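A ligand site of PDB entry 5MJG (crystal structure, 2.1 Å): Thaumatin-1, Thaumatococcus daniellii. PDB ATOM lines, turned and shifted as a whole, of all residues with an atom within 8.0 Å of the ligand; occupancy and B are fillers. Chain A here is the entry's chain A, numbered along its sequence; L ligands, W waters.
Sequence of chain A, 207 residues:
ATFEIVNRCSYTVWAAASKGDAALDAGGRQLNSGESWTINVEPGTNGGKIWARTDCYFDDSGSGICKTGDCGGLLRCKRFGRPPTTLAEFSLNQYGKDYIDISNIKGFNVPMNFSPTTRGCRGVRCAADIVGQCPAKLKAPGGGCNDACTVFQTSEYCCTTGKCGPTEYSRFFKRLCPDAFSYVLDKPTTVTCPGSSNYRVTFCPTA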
ATOM      1  N   GLU A   4       4.105   8.253   2.446  1.00  0.00           N
ATOM      2  CA  GLU A   4       5.034   9.361   2.643  1.00  0.00           C
ATOM      3  C   GLU A   4       5.204  10.092   1.319  1.00  0.00           C
ATOM      4  O   GLU A   4       5.696   9.515   0.346  1.00  0.00           O
ATOM      5  CB  GLU A   4       6.393   8.892   3.160  1.00  0.00           C
ATOM      6  CG  GLU A   4       7.330  10.032   3.493  1.00  0.00           C
ATOM      7  CD  GLU A   4       8.721   9.569   3.857  1.00  0.00           C
ATOM      8  OE1 GLU A   4       9.047   8.392   3.608  1.00  0.00           O
ATOM      9  OE2 GLU A   4       9.494  10.382   4.394  1.00  0.00           O
ATOM     10  N   ILE A   5       4.802  11.363   1.291  1.00  0.00           N
ATOM     11  CA  ILE A   5       4.873  12.176   0.086  1.00  0.00           C
ATOM     12  C   ILE A   5       6.096  13.080   0.201  1.00  0.00           C
ATOM     13  O   ILE A   5       6.157  13.952   1.064  1.00  0.00           O
ATOM     14  CB  ILE A   5       3.584  12.991  -0.102  1.00  0.00           C
ATOM     15  CG1 ILE A   5       2.374  12.050  -0.136  1.00  0.00           C
ATOM     16  CG2 ILE A   5       3.656  13.805  -1.401  1.00  0.00           C
ATOM     17  CD1 ILE A   5       1.032  12.761  -0.087  1.00  0.00           C
ATOM     18  N   VAL A   6       7.075  12.851  -0.674  1.00  0.00           N
ATOM     19  CA  VAL A   6       8.331  13.585  -0.674  1.00  0.00           C
ATOM     20  C   VAL A   6       8.360  14.490  -1.891  1.00  0.00           C
ATOM     21  O   VAL A   6       7.943  14.095  -2.985  1.00  0.00           O
ATOM     22  CB  VAL A   6       9.541  12.637  -0.663  1.00  0.00           C
ATOM     23  CG1 VAL A   6      10.838  13.421  -0.570  1.00  0.00           C
ATOM     24  CG2 VAL A   6       9.430  11.644   0.480  1.00  0.00           C
ATOM     25  N   ASN A   7       8.867  15.709  -1.705  1.00  0.00           N
ATOM     26  CA  ASN A   7       9.048  16.667  -2.798  1.00  0.00           C
ATOM     27  C   ASN A   7      10.546  16.862  -2.990  1.00  0.00           C
ATOM     28  O   ASN A   7      11.184  17.618  -2.251  1.00  0.00           O
ATOM     29  CB  ASN A   7       8.364  17.997  -2.510  1.00  0.00           C
ATOM     30  CG  ASN A   7       8.563  19.001  -3.626  1.00  0.00           C
ATOM     31  OD1 ASN A   7       8.749  18.630  -4.783  1.00  0.00           O
ATOM     32  ND2 ASN A   7       8.533  20.282  -3.288  1.00  0.00           N
ATOM     33  N   ARG A  29      -1.518  19.827   0.830  1.00  0.00           N
ATOM     34  CA  ARG A  29      -0.553  20.569   1.623  1.00  0.00           C
ATOM     35  C   ARG A  29       0.509  21.151   0.697  1.00  0.00           C
ATOM     36  O   ARG A  29       0.743  20.640  -0.397  1.00  0.00           O
ATOM     37  CB  ARG A  29       0.095  19.685   2.691  1.00  0.00           C
ATOM     38  CG  ARG A  29       0.333  20.403   4.013  1.00  0.00           C
ATOM     39  CD  ARG A  29       1.454  19.765   4.801  1.00  0.00           C
ATOM     40  NE  ARG A  29       2.773  20.096   4.258  1.00  0.00           N
ATOM     41  CZ  ARG A  29       3.928  19.789   4.836  1.00  0.00           C
ATOM     42  NH1 ARG A  29       3.945  19.125   5.984  1.00  0.00           N
ATOM     43  NH2 ARG A  29       5.067  20.146   4.265  1.00  0.00           N
ATOM     44  N   GLN A  30       1.144  22.217   1.167  1.00  0.00           N
ATOM     45  CA  GLN A  30       2.277  22.806   0.454  1.00  0.00           C
ATOM     46  C   GLN A  30       3.540  22.036   0.793  1.00  0.00           C
ATOM     47  O   GLN A  30       3.811  21.751   1.973  1.00  0.00           O
ATOM     48  CB  GLN A  30       2.420  24.284   0.824  1.00  0.00           C
ATOM     49  CG  GLN A  30       3.646  24.948   0.218  1.00  0.00           C
ATOM     50  CD  GLN A  30       3.683  26.440   0.480  1.00  0.00           C
ATOM     51  OE1 GLN A  30       2.645  27.066   0.736  1.00  0.00           O
ATOM     52  NE2 GLN A  30       4.872  27.026   0.412  1.00  0.00           N
ATOM     53  N   LEU A  31       4.317  21.684  -0.229  1.00  0.00           N
ATOM     54  CA  LEU A  31       5.558  20.926  -0.064  1.00  0.00           C
ATOM     55  C   LEU A  31       6.711  21.711  -0.696  1.00  0.00           C
ATOM     56  O   LEU A  31       6.881  21.696  -1.922  1.00  0.00           O
ATOM     57  CB  LEU A  31       5.438  19.542  -0.700  1.00  0.00           C
ATOM     58  CG  LEU A  31       5.185  18.387   0.278  1.00  0.00           C
ATOM     59  CD1 LEU A  31       3.939  18.659   1.102  1.00  0.00           C
ATOM     60  CD2 LEU A  31       5.059  17.068  -0.468  1.00  0.00           C
ATOM     61  N   ASN A  32       7.492  22.379   0.138  1.00  0.00           N
ATOM     62  CA  ASN A  32       8.696  23.035  -0.337  1.00  0.00           C
ATOM     63  C   ASN A  32       9.712  21.988  -0.791  1.00  0.00           C
ATOM     64  O   ASN A  32       9.542  20.783  -0.588  1.00  0.00           O
ATOM     65  CB  ASN A  32       9.288  23.916   0.763  1.00  0.00           C
ATOM     66  CG  ASN A  32       8.431  25.123   1.079  1.00  0.00           C
ATOM     67  OD1 ASN A  32       7.347  25.297   0.510  1.00  0.00           O
ATOM     68  ND2 ASN A  32       8.903  25.964   1.990  1.00  0.00           N
ATOM     69  N   SER A  33      10.783  22.471  -1.428  1.00  0.00           N
ATOM     70  CA  SER A  33      11.835  21.577  -1.902  1.00  0.00           C
ATOM     71  C   SER A  33      12.412  20.764  -0.744  1.00  0.00           C
ATOM     72  O   SER A  33      13.029  21.328   0.172  1.00  0.00           O
ATOM     73  CB  SER A  33      12.944  22.380  -2.589  1.00  0.00           C
ATOM     74  OG  SER A  33      13.925  21.515  -3.136  1.00  0.00           O
ATOM     75  N   GLY A  34      12.211  19.454  -0.764  1.00  0.00           N
ATOM     76  CA  GLY A  34      12.770  18.559   0.231  1.00  0.00           C
ATOM     77  C   GLY A  34      11.826  18.193   1.372  1.00  0.00           C
ATOM     78  O   GLY A  34      12.185  17.342   2.186  1.00  0.00           O
ATOM     79  N   GLU A  35      10.648  18.809   1.443  1.00  0.00           N
ATOM     80  CA  GLU A  35       9.712  18.539   2.528  1.00  0.00           C
ATOM     81  C   GLU A  35       8.953  17.237   2.278  1.00  0.00           C
ATOM     82  O   GLU A  35       8.591  16.904   1.149  1.00  0.00           O
ATOM     83  CB  GLU A  35       8.712  19.683   2.675  1.00  0.00           C
ATOM     84  CG  GLU A  35       9.294  20.925   3.331  1.00  0.00           C
ATOM     85  CD  GLU A  35       8.259  21.982   3.640  1.00  0.00           C
ATOM     86  OE1 GLU A  35       7.110  21.868   3.163  1.00  0.00           O
ATOM     87  OE2 GLU A  35       8.596  22.938   4.379  1.00  0.00           O
ATOM     88  N   SER A  36       8.724  16.503   3.362  1.00  0.00           N
ATOM     89  CA  SER A  36       7.988  15.242   3.319  1.00  0.00           C
ATOM     90  C   SER A  36       6.653  15.407   4.044  1.00  0.00           C
ATOM     91  O   SER A  36       6.532  16.180   4.998  1.00  0.00           O
ATOM     92  CB  SER A  36       8.800  14.111   3.954  1.00  0.00           C
ATOM     93  OG  SER A  36      10.092  14.022   3.370  1.00  0.00           O
ATOM     94  N   TRP A  37       5.638  14.686   3.564  1.00  0.00           N
ATOM     95  CA  TRP A  37       4.303  14.732   4.143  1.00  0.00           C
ATOM     96  C   TRP A  37       3.829  13.311   4.373  1.00  0.00           C
ATOM     97  O   TRP A  37       3.717  12.529   3.430  1.00  0.00           O
ATOM     98  CB  TRP A  37       3.334  15.481   3.217  1.00  0.00           C
ATOM     99  CG  TRP A  37       1.942  15.603   3.764  1.00  0.00           C
ATOM    100  CD1 TRP A  37       1.555  15.571   5.064  1.00  0.00           C
ATOM    101  CD2 TRP A  37       0.738  15.780   2.996  1.00  0.00           C
ATOM    102  NE1 TRP A  37       0.200  15.716   5.164  1.00  0.00           N
ATOM    103  CE2 TRP A  37      -0.331  15.845   3.910  1.00  0.00           C
ATOM    104  CE3 TRP A  37       0.471  15.885   1.626  1.00  0.00           C
ATOM    105  CZ2 TRP A  37      -1.645  16.014   3.499  1.00  0.00           C
ATOM    106  CZ3 TRP A  37      -0.838  16.059   1.222  1.00  0.00           C
ATOM    107  CH2 TRP A  37      -1.888  16.117   2.157  1.00  0.00           C
ATOM    108  N   THR A  38       3.548  12.981   5.638  1.00  0.00           N
ATOM    109  CA  THR A  38       3.058  11.656   6.001  1.00  0.00           C
ATOM    110  C   THR A  38       1.554  11.728   6.190  1.00  0.00           C
ATOM    111  O   THR A  38       1.045  12.596   6.904  1.00  0.00           O
ATOM    112  CB  THR A  38       3.736  11.165   7.283  1.00  0.00           C
ATOM    113  OG1 THR A  38       5.149  11.158   7.099  1.00  0.00           O
ATOM    114  CG2 THR A  38       3.268   9.763   7.631  1.00  0.00           C
HETATM  115  O1  LIG L   1       6.979  19.293   9.303  1.00  0.00           O
HETATM  116  O2  LIG L   1       5.281  18.760   8.055  1.00  0.00           O
HETATM  117  C1  LIG L   1       6.525  18.851   8.216  1.00  0.00           C
HETATM  118  C2  LIG L   1       7.456  18.418   7.091  1.00  0.00           C
HETATM  119  O3  LIG L   1       7.516  19.443   6.131  1.00  0.00           O
HETATM  120  C3  LIG L   1       8.864  18.127   7.619  1.00  0.00           C
HETATM  121  O4  LIG L   1       8.933  16.774   7.968  1.00  0.00           O
HETATM  122  C4  LIG L   1       9.904  18.417   6.541  1.00  0.00           C
HETATM  123  O5  LIG L   1      10.360  19.586   6.397  1.00  0.00           O
HETATM  124  O6  LIG L   1      10.313  17.482   5.795  1.00  0.00           O
HETATM  125  O   HOH W   1      11.879  15.907   4.234  1.00  0.00           O
HETATM  126  O   HOH W   2      10.008  22.154   7.026  1.00  0.00           O
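O2 of the ligand lies within salt-bridge range of NH1 of Arg 29, 2.5 Å away. O6 of the ligand is in hydrogen-bond range of N of Ser 36 (3.1 Å).
NH2 of Arg 29 lies within salt-bridge range of OE1 of Glu 35 (2.9 Å). The side-chain carboxylate (OE1) of Glu 35 lies within hydrogen-bond range of the backbone NH (N) of Asn 32, 3.1 Å away. O of Glu 35 lies within hydrogen-bond range of N of Asn 7 (3.1 Å).
Merely in contact with the ligand: Glu 35. Three residues have an atom within 4 Å of the ligand: Arg 29, Glu 35 and Ser 36. The nearest printed residue that does not touch the ligand is Gly 34 (4.1 Å).
Water W2 lies within hydrogen-bond range of O5 of the ligand and OE2 of Glu 35. Water W1 lies within hydrogen-bond range of the backbone carbonyl oxygen (O) of Gly 34, an oxygen (O6) of the ligand and the side-chain hydroxyl (OG) of Ser 36.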
